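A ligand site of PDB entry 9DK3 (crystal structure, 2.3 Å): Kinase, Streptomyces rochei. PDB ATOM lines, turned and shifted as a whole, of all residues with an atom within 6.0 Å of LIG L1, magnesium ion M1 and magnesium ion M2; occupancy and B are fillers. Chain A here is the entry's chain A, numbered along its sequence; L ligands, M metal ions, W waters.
A nitrogen (N3) of LIG L1 is in hydrogen-bond range of the backbone carbonyl oxygen of Arg 119. N of Arg 51 is in hydrogen-bond range of O2 of LIG L1 (3.3 Å). An oxygen (O2) of LIG L1 is in hydrogen-bond range of the side-chain amide nitrogen (ND2) of Asn 54, 3.4 Å away. N of Val 121 sits at hydrogen-bond distance from N4 of LIG L1 (3.0 Å). O2 of LIG L1 sits at hydrogen-bond distance from N of Asn 52. An oxygen (O2) of LIG L1 is in hydrogen-bond range of the side-chain amide nitrogen (ND2) of Asn 52. NZ of Lys 68 lies within salt-bridge range of O4 of LIG L1, at 2.8 Å. The backbone carbonyl oxygen of Asp 227 lies within hydrogen-bond range of an oxygen (O9) of LIG L1 (2.5 Å).
The guanidinium group of Arg 119 lies within hydrogen-bond range of the backbone carbonyl oxygen of Pro 104 (2.6 Å). The guanidinium group of Arg 225 lies within salt-bridge range of the side-chain carboxylate of Asp 223 (3.3 Å). The side-chain carboxylate of Glu 245 is in salt-bridge range of the guanidinium group of Arg 51 (3.2 Å). The side-chain carboxylate (OE1) of Glu 129 sits at hydrogen-bond distance from the backbone NH (N) of Ser 126 (3.1 Å). The backbone NH of Phe 66 sits at hydrogen-bond distance from the backbone carbonyl oxygen of His 118, at 2.7 Å. The backbone NH (N) of Val 242 sits at hydrogen-bond distance from the backbone carbonyl oxygen (O) of Gln 228. OE2 of Glu 245 sits at hydrogen-bond distance from ND2 of Asn 52. OD1 of Asp 243 sits close to NZ of Lys 68, 2.9 Å away.
CB of Phe 48 touches O8 of LIG L1, at 3.9 Å. O of Gly 49 touches O2 of LIG L1 (3.7 Å). CA of Gly 50 touches O2 of LIG L1 (3.2 Å). CZ of Phe 66 touches C6 of LIG L1, 3.4 Å away. Pro 104 touches LIG L1 (CB to N3, 3.7 Å). CD1 of Leu 120 touches C9 of LIG L1, 3.4 Å away. Ala 124 touches LIG L1. Ser 126 touches LIG L1 (CB to O10, 3.7 Å). Ile 230 touches LIG L1 (CG2 to C4, 3.5 Å). 19 residues have an atom within 4 Å of LIG L1: Phe 48, Gly 49, Gly 50, Arg 51, Asn 52, Asn 54, Phe 66, Lys 68, Pro 104, Arg 119, Leu 120, Val 121, Ala 124, Ser 126, Asp 227, Gln 228, Ile 230, Asp 243 and Glu 245.
Residues that only touch magnesium ion M1: Arg 225. Within 4 Å of magnesium ion M1: Arg 225, Gln 228 and Asp 243. Along chain A the residues within 4 Å of magnesium ion M1 span positions 225 to 243.
Merely in contact with magnesium ion M2: Lys 68 (3.8 Å) and Asn 52 (3.9 Å). Four residues have an atom within 4 Å of magnesium ion M2: Asn 52, Lys 68, Asp 243 and Glu 245. The nearest printed residue that does not touch magnesium ion M2 is Arg 51 (4.03 Å).
Magnesium ion M1 is bound by an oxygen (O5) of LIG L1 (2.0 Å), the side-chain amide oxygen (OE1) of Gln 228 (2.0 Å), an oxygen (O4) of LG2 L2 (2.0 Å), an oxygen (O1) of LIG L1 (2.0 Å), the side-chain carboxylate (OD2) of Asp 243 (2.1 Å) and water W2 (2.2 Å).
Magnesium ion M2 is bound by the side-chain carboxylate (OD2) of Asp 243 (1.8 Å), the side-chain carboxylate (OD1) of Asp 243 (1.9 Å), an oxygen (O3) of LIG L1 (2.0 Å), the side-chain carboxylate (OE1) of Glu 245 (2.0 Å), an oxygen (O3) of LG2 L2 (2.0 Å) and water W1 (2.4 Å).
Water W2 bridges an oxygen (O9) of LIG L1 (2.9 Å) and the side-chain carboxylate (OD2) of Asp 227 (3.3 Å). Water W1 lies within hydrogen-bond range of the side-chain carboxylate (OD2) of Asp 223 (2.6 Å) and the guanidinium group (NH1) of Arg 51 (3.1 Å).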
ATOM      1  N   PHE A  48       0.789   8.732 -15.716  1.00  0.00           N
ATOM      2  CA  PHE A  48       0.135   8.487 -14.424  1.00  0.00           C
ATOM      3  C   PHE A  48       0.891   7.343 -13.720  1.00  0.00           C
ATOM      4  O   PHE A  48       1.831   6.771 -14.294  1.00  0.00           O
ATOM      5  CB  PHE A  48      -1.367   8.247 -14.639  1.00  0.00           C
ATOM      6  N   GLY A  49       0.495   7.030 -12.470  1.00  0.00           N
ATOM      7  CA  GLY A  49       1.295   6.238 -11.534  1.00  0.00           C
ATOM      8  C   GLY A  49       1.116   4.727 -11.682  1.00  0.00           C
ATOM      9  O   GLY A  49       0.681   4.252 -12.722  1.00  0.00           O
ATOM     10  N   GLY A  50       1.508   3.977 -10.634  1.00  0.00           N
ATOM     11  CA  GLY A  50       1.400   2.520 -10.573  1.00  0.00           C
ATOM     12  C   GLY A  50       2.647   1.806 -11.107  1.00  0.00           C
ATOM     13  O   GLY A  50       3.570   2.446 -11.629  1.00  0.00           O
ATOM     14  N   ARG A  51       2.737   0.503 -10.986  1.00  0.00           N
ATOM     15  CA  ARG A  51       3.960  -0.275 -11.363  1.00  0.00           C
ATOM     16  C   ARG A  51       4.038  -0.488 -12.869  1.00  0.00           C
ATOM     17  O   ARG A  51       4.967  -1.167 -13.311  1.00  0.00           O
ATOM     18  CB  ARG A  51       3.839  -1.670 -10.751  1.00  0.00           C
ATOM     19  CG  ARG A  51       2.463  -2.288 -10.927  1.00  0.00           C
ATOM     20  CD  ARG A  51       2.455  -3.787 -10.736  1.00  0.00           C
ATOM     21  NE  ARG A  51       1.272  -4.238 -10.021  1.00  0.00           N
ATOM     22  CZ  ARG A  51       0.495  -5.254 -10.407  1.00  0.00           C
ATOM     23  NH1 ARG A  51      -0.554  -5.597  -9.692  1.00  0.00           N
ATOM     24  NH2 ARG A  51       0.789  -5.919 -11.517  1.00  0.00           N
ATOM     25  N   ASN A  52       3.073   0.055 -13.622  1.00  0.00           N
ATOM     26  CA  ASN A  52       2.987  -0.094 -15.065  1.00  0.00           C
ATOM     27  C   ASN A  52       3.209   1.271 -15.735  1.00  0.00           C
ATOM     28  O   ASN A  52       2.944   2.296 -15.105  1.00  0.00           O
ATOM     29  CB  ASN A  52       1.596  -0.608 -15.417  1.00  0.00           C
ATOM     30  CG  ASN A  52       1.302  -1.956 -14.789  1.00  0.00           C
ATOM     31  OD1 ASN A  52       1.996  -2.915 -15.076  1.00  0.00           O
ATOM     32  ND2 ASN A  52       0.275  -2.037 -13.942  1.00  0.00           N
ATOM     33  N   ASP A  53       3.623   1.245 -16.995  1.00  0.00           N
ATOM     34  CA  ASP A  53       3.733   2.505 -17.773  1.00  0.00           C
ATOM     35  C   ASP A  53       2.340   2.884 -18.266  1.00  0.00           C
ATOM     36  O   ASP A  53       1.724   2.083 -18.958  1.00  0.00           O
ATOM     37  CB  ASP A  53       4.729   2.394 -18.933  1.00  0.00           C
ATOM     38  CG  ASP A  53       6.180   2.424 -18.495  1.00  0.00           C
ATOM     39  OD1 ASP A  53       6.503   3.189 -17.575  1.00  0.00           O
ATOM     40  OD2 ASP A  53       6.982   1.671 -19.089  1.00  0.00           O
ATOM     41  N   ASN A  54       1.892   4.076 -17.903  1.00  0.00           N
ATOM     42  CA  ASN A  54       0.527   4.490 -18.271  1.00  0.00           C
ATOM     43  C   ASN A  54       0.567   5.875 -18.914  1.00  0.00           C
ATOM     44  O   ASN A  54       1.433   6.671 -18.561  1.00  0.00           O
ATOM     45  CB  ASN A  54      -0.378   4.465 -17.037  1.00  0.00           C
ATOM     46  CG  ASN A  54      -0.348   3.149 -16.298  1.00  0.00           C
ATOM     47  OD1 ASN A  54      -0.192   2.095 -16.915  1.00  0.00           O
ATOM     48  ND2 ASN A  54      -0.502   3.188 -14.990  1.00  0.00           N
ATOM     49  N   PHE A  66      -7.247   6.757 -21.383  1.00  0.00           N
ATOM     50  CA  PHE A  66      -6.283   6.275 -20.404  1.00  0.00           C
ATOM     51  C   PHE A  66      -5.652   5.004 -20.962  1.00  0.00           C
ATOM     52  O   PHE A  66      -6.348   4.007 -21.161  1.00  0.00           O
ATOM     53  CB  PHE A  66      -6.961   6.018 -19.058  1.00  0.00           C
ATOM     54  CG  PHE A  66      -5.995   5.481 -18.036  1.00  0.00           C
ATOM     55  CD1 PHE A  66      -5.169   6.357 -17.319  1.00  0.00           C
ATOM     56  CD2 PHE A  66      -5.797   4.110 -17.905  1.00  0.00           C
ATOM     57  CE1 PHE A  66      -4.222   5.856 -16.436  1.00  0.00           C
ATOM     58  CE2 PHE A  66      -4.855   3.615 -17.018  1.00  0.00           C
ATOM     59  CZ  PHE A  66      -4.047   4.492 -16.298  1.00  0.00           C
ATOM     60  N   LYS A  68      -2.902   1.901 -20.599  1.00  0.00           N
ATOM     61  CA  LYS A  68      -2.074   1.109 -19.676  1.00  0.00           C
ATOM     62  C   LYS A  68      -1.299   0.064 -20.467  1.00  0.00           C
ATOM     63  O   LYS A  68      -1.890  -0.562 -21.338  1.00  0.00           O
ATOM     64  CB  LYS A  68      -2.945   0.417 -18.635  1.00  0.00           C
ATOM     65  CG  LYS A  68      -2.281  -0.756 -17.920  1.00  0.00           C
ATOM     66  CD  LYS A  68      -3.165  -1.363 -16.856  1.00  0.00           C
ATOM     67  CE  LYS A  68      -3.196  -0.551 -15.580  1.00  0.00           C
ATOM     68  NZ  LYS A  68      -3.931  -1.254 -14.503  1.00  0.00           N
ATOM     69  N   PRO A 104     -14.932   3.120 -16.189  1.00  0.00           N
ATOM     70  CA  PRO A 104     -14.703   4.202 -17.162  1.00  0.00           C
ATOM     71  C   PRO A 104     -15.149   3.933 -18.617  1.00  0.00           C
ATOM     72  O   PRO A 104     -15.623   4.825 -19.334  1.00  0.00           O
ATOM     73  CB  PRO A 104     -13.191   4.316 -17.063  1.00  0.00           C
ATOM     74  CG  PRO A 104     -12.883   4.023 -15.617  1.00  0.00           C
ATOM     75  CD  PRO A 104     -13.793   2.862 -15.304  1.00  0.00           C
ATOM     76  N   HIS A 118      -8.780   2.787 -22.151  1.00  0.00           N
ATOM     77  CA  HIS A 118     -10.044   3.101 -21.531  1.00  0.00           C
ATOM     78  C   HIS A 118     -10.348   4.572 -21.760  1.00  0.00           C
ATOM     79  O   HIS A 118      -9.420   5.349 -21.953  1.00  0.00           O
ATOM     80  CB  HIS A 118     -10.021   2.857 -19.999  1.00  0.00           C
ATOM     81  CG  HIS A 118     -10.084   1.433 -19.557  1.00  0.00           C
ATOM     82  ND1 HIS A 118      -8.993   0.575 -19.654  1.00  0.00           N
ATOM     83  CD2 HIS A 118     -11.120   0.714 -19.016  1.00  0.00           C
ATOM     84  CE1 HIS A 118      -9.357  -0.625 -19.178  1.00  0.00           C
ATOM     85  NE2 HIS A 118     -10.683  -0.572 -18.820  1.00  0.00           N
ATOM     86  N   ARG A 119     -11.628   4.912 -21.624  1.00  0.00           N
ATOM     87  CA  ARG A 119     -12.112   6.276 -21.521  1.00  0.00           C
ATOM     88  C   ARG A 119     -11.401   6.933 -20.332  1.00  0.00           C
ATOM     89  O   ARG A 119     -11.256   6.313 -19.284  1.00  0.00           O
ATOM     90  CB  ARG A 119     -13.650   6.236 -21.398  1.00  0.00           C
ATOM     91  CG  ARG A 119     -14.391   7.568 -21.289  1.00  0.00           C
ATOM     92  CD  ARG A 119     -15.894   7.457 -21.040  1.00  0.00           C
ATOM     93  NE  ARG A 119     -16.322   7.363 -19.631  1.00  0.00           N
ATOM     94  CZ  ARG A 119     -16.197   8.329 -18.723  1.00  0.00           C
ATOM     95  NH1 ARG A 119     -15.508   9.418 -18.993  1.00  0.00           N
ATOM     96  NH2 ARG A 119     -16.738   8.209 -17.524  1.00  0.00           N
ATOM     97  N   LEU A 120     -10.891   8.157 -20.515  1.00  0.00           N
ATOM     98  CA  LEU A 120     -10.383   8.962 -19.413  1.00  0.00           C
ATOM     99  C   LEU A 120     -11.563   9.478 -18.607  1.00  0.00           C
ATOM    100  O   LEU A 120     -12.603   9.788 -19.168  1.00  0.00           O
ATOM    101  CB  LEU A 120      -9.535  10.118 -19.935  1.00  0.00           C
ATOM    102  CG  LEU A 120      -8.808  10.926 -18.856  1.00  0.00           C
ATOM    103  CD1 LEU A 120      -7.927  10.047 -17.997  1.00  0.00           C
ATOM    104  CD2 LEU A 120      -7.937  12.014 -19.483  1.00  0.00           C
ATOM    105  N   VAL A 121     -11.428   9.460 -17.260  1.00  0.00           N
ATOM    106  CA  VAL A 121     -12.359  10.154 -16.374  1.00  0.00           C
ATOM    107  C   VAL A 121     -11.839  11.586 -16.224  1.00  0.00           C
ATOM    108  O   VAL A 121     -10.727  11.776 -15.739  1.00  0.00           O
ATOM    109  CB  VAL A 121     -12.545   9.460 -15.014  1.00  0.00           C
ATOM    110  CG1 VAL A 121     -13.346  10.315 -14.043  1.00  0.00           C
ATOM    111  CG2 VAL A 121     -13.225   8.110 -15.164  1.00  0.00           C
ATOM    112  N   PRO A 122     -12.588  12.613 -16.700  1.00  0.00           N
ATOM    113  CA  PRO A 122     -12.112  14.001 -16.703  1.00  0.00           C
ATOM    114  C   PRO A 122     -11.910  14.540 -15.288  1.00  0.00           C
ATOM    115  O   PRO A 122     -12.842  14.445 -14.465  1.00  0.00           O
ATOM    116  CB  PRO A 122     -13.233  14.785 -17.398  1.00  0.00           C
ATOM    117  CG  PRO A 122     -14.480  13.939 -17.191  1.00  0.00           C
ATOM    118  CD  PRO A 122     -13.985  12.504 -17.172  1.00  0.00           C
ATOM    119  N   ALA A 124      -9.772  13.560 -12.845  1.00  0.00           N
ATOM    120  CA  ALA A 124      -9.792  12.413 -11.952  1.00  0.00           C
ATOM    121  C   ALA A 124      -9.013  12.784 -10.698  1.00  0.00           C
ATOM    122  O   ALA A 124      -7.900  13.276 -10.847  1.00  0.00           O
ATOM    123  CB  ALA A 124      -9.150  11.236 -12.641  1.00  0.00           C
ATOM    124  N   ARG A 125      -9.616  12.577  -9.517  1.00  0.00           N
ATOM    125  CA  ARG A 125      -8.881  12.621  -8.255  1.00  0.00           C
ATOM    126  C   ARG A 125      -8.881  11.215  -7.623  1.00  0.00           C
ATOM    127  O   ARG A 125      -9.927  10.544  -7.531  1.00  0.00           O
ATOM    128  CB  ARG A 125      -9.480  13.778  -7.423  1.00  0.00           C
ATOM    129  CG  ARG A 125      -8.521  14.381  -6.396  1.00  0.00           C
ATOM    130  CD  ARG A 125      -9.044  15.573  -5.600  1.00  0.00           C
ATOM    131  NE  ARG A 125      -8.796  16.854  -6.262  1.00  0.00           N
ATOM    132  CZ  ARG A 125      -8.085  17.853  -5.751  1.00  0.00           C
ATOM    133  NH1 ARG A 125      -8.105  19.058  -6.308  1.00  0.00           N
ATOM    134  NH2 ARG A 125      -7.361  17.656  -4.662  1.00  0.00           N
ATOM    135  N   SER A 126      -7.699  10.700  -7.234  1.00  0.00           N
ATOM    136  CA  SER A 126      -7.666   9.332  -6.709  1.00  0.00           C
ATOM    137  C   SER A 126      -8.147   9.316  -5.264  1.00  0.00           C
ATOM    138  O   SER A 126      -8.131  10.334  -4.576  1.00  0.00           O
ATOM    139  CB  SER A 126      -6.300   8.694  -6.869  1.00  0.00           C
ATOM    140  OG  SER A 126      -5.461   9.001  -5.772  1.00  0.00           O
ATOM    141  N   GLU A 129      -5.556  10.773  -2.782  1.00  0.00           N
ATOM    142  CA  GLU A 129      -5.519  12.236  -2.714  1.00  0.00           C
ATOM    143  C   GLU A 129      -6.671  12.748  -1.851  1.00  0.00           C
ATOM    144  O   GLU A 129      -6.493  13.634  -1.018  1.00  0.00           O
ATOM    145  CB  GLU A 129      -5.654  12.874  -4.102  1.00  0.00           C
ATOM    146  CG  GLU A 129      -4.492  12.584  -5.062  1.00  0.00           C
ATOM    147  CD  GLU A 129      -4.692  13.093  -6.489  1.00  0.00           C
ATOM    148  OE1 GLU A 129      -5.088  12.278  -7.390  1.00  0.00           O
ATOM    149  OE2 GLU A 129      -4.460  14.303  -6.717  1.00  0.00           O
ATOM    150  N   ASP A 223      -6.722  -6.364  -5.082  1.00  0.00           N
ATOM    151  CA  ASP A 223      -5.612  -5.386  -5.002  1.00  0.00           C
ATOM    152  C   ASP A 223      -6.187  -4.032  -4.621  1.00  0.00           C
ATOM    153  O   ASP A 223      -5.762  -3.033  -5.188  1.00  0.00           O
ATOM    154  CB  ASP A 223      -4.888  -5.262  -6.329  1.00  0.00           C
ATOM    155  CG  ASP A 223      -3.565  -4.530  -6.279  1.00  0.00           C
ATOM    156  OD1 ASP A 223      -2.852  -4.690  -5.281  1.00  0.00           O
ATOM    157  OD2 ASP A 223      -3.278  -3.829  -7.242  1.00  0.00           O
ATOM    158  N   ARG A 225      -6.793  -0.609  -2.915  1.00  0.00           N
ATOM    159  CA  ARG A 225      -6.390   0.487  -2.056  1.00  0.00           C
ATOM    160  C   ARG A 225      -7.169   1.736  -2.458  1.00  0.00           C
ATOM    161  O   ARG A 225      -7.840   1.753  -3.490  1.00  0.00           O
ATOM    162  CB  ARG A 225      -4.905   0.763  -2.239  1.00  0.00           C
ATOM    163  CG  ARG A 225      -4.019  -0.416  -1.892  1.00  0.00           C
ATOM    164  CD  ARG A 225      -2.584   0.002  -2.048  1.00  0.00           C
ATOM    165  NE  ARG A 225      -2.307   0.465  -3.400  1.00  0.00           N
ATOM    166  CZ  ARG A 225      -2.096  -0.312  -4.449  1.00  0.00           C
ATOM    167  NH1 ARG A 225      -2.090  -1.637  -4.340  1.00  0.00           N
ATOM    168  NH2 ARG A 225      -1.880   0.265  -5.617  1.00  0.00           N
ATOM    169  N   ASP A 227      -5.957   4.386  -3.844  1.00  0.00           N
ATOM    170  CA  ASP A 227      -5.441   4.869  -5.140  1.00  0.00           C
ATOM    171  C   ASP A 227      -6.032   4.081  -6.315  1.00  0.00           C
ATOM    172  O   ASP A 227      -5.751   4.448  -7.451  1.00  0.00           O
ATOM    173  CB  ASP A 227      -3.917   4.808  -5.143  1.00  0.00           C
ATOM    174  CG  ASP A 227      -3.353   3.537  -4.535  1.00  0.00           C
ATOM    175  OD1 ASP A 227      -3.220   3.493  -3.298  1.00  0.00           O
ATOM    176  OD2 ASP A 227      -3.065   2.599  -5.293  1.00  0.00           O
ATOM    177  N   GLN A 228      -6.802   3.027  -6.036  1.00  0.00           N
ATOM    178  CA  GLN A 228      -7.483   2.236  -7.091  1.00  0.00           C
ATOM    179  C   GLN A 228      -8.874   2.814  -7.271  1.00  0.00           C
ATOM    180  O   GLN A 228      -9.589   2.335  -8.141  1.00  0.00           O
ATOM    181  CB  GLN A 228      -7.435   0.754  -6.716  1.00  0.00           C
ATOM    182  CG  GLN A 228      -6.072   0.289  -6.229  1.00  0.00           C
ATOM    183  CD  GLN A 228      -5.163  -0.120  -7.367  1.00  0.00           C
ATOM    184  OE1 GLN A 228      -4.699   0.699  -8.147  1.00  0.00           O
ATOM    185  NE2 GLN A 228      -4.906  -1.416  -7.458  1.00  0.00           N
ATOM    186  N   PHE A 229      -9.247   3.796  -6.458  1.00  0.00           N
ATOM    187  CA  PHE A 229     -10.504   4.525  -6.641  1.00  0.00           C
ATOM    188  C   PHE A 229     -10.221   5.895  -7.231  1.00  0.00           C
ATOM    189  O   PHE A 229      -9.164   6.484  -6.972  1.00  0.00           O
ATOM    190  CB  PHE A 229     -11.289   4.724  -5.345  1.00  0.00           C
ATOM    191  CG  PHE A 229     -11.860   3.485  -4.714  1.00  0.00           C
ATOM    192  CD1 PHE A 229     -11.152   2.807  -3.734  1.00  0.00           C
ATOM    193  CD2 PHE A 229     -13.148   3.097  -4.980  1.00  0.00           C
ATOM    194  CE1 PHE A 229     -11.708   1.718  -3.085  1.00  0.00           C
ATOM    195  CE2 PHE A 229     -13.706   2.001  -4.342  1.00  0.00           C
ATOM    196  CZ  PHE A 229     -12.987   1.300  -3.401  1.00  0.00           C
ATOM    197  N   ILE A 230     -11.113   6.312  -8.136  1.00  0.00           N
ATOM    198  CA  ILE A 230     -11.054   7.629  -8.737  1.00  0.00           C
ATOM    199  C   ILE A 230     -12.446   8.239  -8.691  1.00  0.00           C
ATOM    200  O   ILE A 230     -13.475   7.549  -8.700  1.00  0.00           O
ATOM    201  CB  ILE A 230     -10.476   7.646 -10.165  1.00  0.00           C
ATOM    202  CG1 ILE A 230     -11.309   6.842 -11.151  1.00  0.00           C
ATOM    203  CG2 ILE A 230      -9.032   7.202 -10.176  1.00  0.00           C
ATOM    204  CD1 ILE A 230     -10.774   6.910 -12.553  1.00  0.00           C
ATOM    205  N   VAL A 242     -10.804   1.024 -10.103  1.00  0.00           N
ATOM    206  CA  VAL A 242      -9.989   0.660 -11.305  1.00  0.00           C
ATOM    207  C   VAL A 242      -8.860  -0.318 -10.962  1.00  0.00           C
ATOM    208  O   VAL A 242      -8.848  -0.780  -9.832  1.00  0.00           O
ATOM    209  CB  VAL A 242      -9.452   1.963 -11.920  1.00  0.00           C
ATOM    210  CG1 VAL A 242     -10.548   2.999 -12.102  1.00  0.00           C
ATOM    211  CG2 VAL A 242      -8.293   2.551 -11.123  1.00  0.00           C
ATOM    212  N   ASP A 243      -7.953  -0.618 -11.905  1.00  0.00           N
ATOM    213  CA  ASP A 243      -6.800  -1.554 -11.730  1.00  0.00           C
ATOM    214  C   ASP A 243      -7.280  -2.963 -11.423  1.00  0.00           C
ATOM    215  O   ASP A 243      -7.050  -3.422 -10.315  1.00  0.00           O
ATOM    216  CB  ASP A 243      -5.732  -1.051 -10.751  1.00  0.00           C
ATOM    217  CG  ASP A 243      -4.329  -1.578 -10.999  1.00  0.00           C
ATOM    218  OD1 ASP A 243      -4.167  -2.391 -11.895  1.00  0.00           O
ATOM    219  OD2 ASP A 243      -3.435  -1.154 -10.279  1.00  0.00           O
ATOM    220  N   TRP A 244      -7.841  -3.636 -12.422  1.00  0.00           N
ATOM    221  CA  TRP A 244      -8.448  -4.975 -12.233  1.00  0.00           C
ATOM    222  C   TRP A 244      -7.462  -6.069 -12.634  1.00  0.00           C
ATOM    223  O   TRP A 244      -7.908  -7.167 -12.939  1.00  0.00           O
ATOM    224  CB  TRP A 244      -9.760  -5.020 -13.010  1.00  0.00           C
ATOM    225  CG  TRP A 244     -10.788  -4.081 -12.455  1.00  0.00           C
ATOM    226  CD1 TRP A 244     -11.017  -2.794 -12.834  1.00  0.00           C
ATOM    227  CD2 TRP A 244     -11.712  -4.364 -11.400  1.00  0.00           C
ATOM    228  NE1 TRP A 244     -12.038  -2.264 -12.089  1.00  0.00           N
ATOM    229  CE2 TRP A 244     -12.476  -3.205 -11.199  1.00  0.00           C
ATOM    230  CE3 TRP A 244     -11.978  -5.483 -10.602  1.00  0.00           C
ATOM    231  CZ2 TRP A 244     -13.491  -3.125 -10.246  1.00  0.00           C
ATOM    232  CZ3 TRP A 244     -12.971  -5.411  -9.656  1.00  0.00           C
ATOM    233  CH2 TRP A 244     -13.710  -4.246  -9.481  1.00  0.00           C
ATOM    234  N   GLU A 245      -6.173  -5.771 -12.593  1.00  0.00           N
ATOM    235  CA  GLU A 245      -5.144  -6.761 -12.916  1.00  0.00           C
ATOM    236  C   GLU A 245      -5.195  -8.038 -12.070  1.00  0.00           C
ATOM    237  O   GLU A 245      -4.580  -9.018 -12.473  1.00  0.00           O
ATOM    238  CB  GLU A 245      -3.768  -6.186 -12.610  1.00  0.00           C
ATOM    239  CG  GLU A 245      -3.413  -5.050 -13.529  1.00  0.00           C
ATOM    240  CD  GLU A 245      -1.995  -4.617 -13.256  1.00  0.00           C
ATOM    241  OE1 GLU A 245      -1.794  -3.886 -12.266  1.00  0.00           O
ATOM    242  OE2 GLU A 245      -1.112  -5.077 -13.979  1.00  0.00           O
HETATM  243  P1  LIG L   1      -1.347   0.339 -12.152  1.00  0.00           P
HETATM  244  O1  LIG L   1      -1.512   0.699 -10.667  1.00  0.00           O
HETATM  245  O2  LIG L   1      -0.048   0.656 -12.748  1.00  0.00           O
HETATM  246  O3  LIG L   1      -1.704  -1.049 -12.469  1.00  0.00           O
HETATM  247  P2  LIG L   1      -3.945   1.727 -12.457  1.00  0.00           P
HETATM  248  O4  LIG L   1      -4.989   0.998 -13.276  1.00  0.00           O
HETATM  249  O5  LIG L   1      -3.967   1.616 -10.945  1.00  0.00           O
HETATM  250  O6  LIG L   1      -2.438   1.343 -12.835  1.00  0.00           O
HETATM  251  O7  LIG L   1      -3.987   3.272 -12.857  1.00  0.00           O
HETATM  252  C1  LIG L   1      -2.979   4.161 -12.368  1.00  0.00           C
HETATM  253  C2  LIG L   1      -3.670   5.381 -11.818  1.00  0.00           C
HETATM  254  O8  LIG L   1      -4.142   6.205 -12.918  1.00  0.00           O
HETATM  255  C3  LIG L   1      -4.917   5.039 -11.001  1.00  0.00           C
HETATM  256  O9  LIG L   1      -4.541   4.792  -9.656  1.00  0.00           O
HETATM  257  C4  LIG L   1      -5.788   6.283 -11.196  1.00  0.00           C
HETATM  258  O10 LIG L   1      -5.451   7.208 -10.187  1.00  0.00           O
HETATM  259  C5  LIG L   1      -5.431   6.701 -12.627  1.00  0.00           C
HETATM  260  N1  LIG L   1      -6.387   6.212 -13.635  1.00  0.00           N
HETATM  261  C6  LIG L   1      -6.550   4.914 -14.071  1.00  0.00           C
HETATM  262  N2  LIG L   1      -7.537   4.751 -14.912  1.00  0.00           N
HETATM  263  C7  LIG L   1      -8.050   6.031 -15.074  1.00  0.00           C
HETATM  264  C8  LIG L   1      -9.071   6.533 -15.910  1.00  0.00           C
HETATM  265  N3  LIG L   1      -9.834   5.775 -16.698  1.00  0.00           N
HETATM  266  N4  LIG L   1      -9.356   7.858 -15.807  1.00  0.00           N
HETATM  267  C9  LIG L   1      -8.604   8.611 -14.979  1.00  0.00           C
HETATM  268  N5  LIG L   1      -7.594   8.256 -14.169  1.00  0.00           N
HETATM  269  C10 LIG L   1      -7.378   6.931 -14.260  1.00  0.00           C
HETATM  270  P1  LG2 L   2      -0.808  -1.699  -8.360  1.00  0.00           P
HETATM  271  O1  LG2 L   2      -1.218  -2.673  -7.282  1.00  0.00           O
HETATM  272  O2  LG2 L   2       0.667  -1.341  -8.039  1.00  0.00           O
HETATM  273  O3  LG2 L   2      -0.955  -2.325  -9.838  1.00  0.00           O
HETATM  274  O4  LG2 L   2      -1.753  -0.402  -8.313  1.00  0.00           O
HETATM  275 MG    MG M   1      -3.108   0.672  -9.389  1.00  0.00          MG
HETATM  276 MG    MG M   2      -2.439  -2.357 -11.183  1.00  0.00          MG
HETATM  277  O   HOH W   1      -3.319  -4.133  -9.847  1.00  0.00           O
HETATM  278  O   HOH W   2      -2.871   2.648  -8.573  1.00  0.00           O
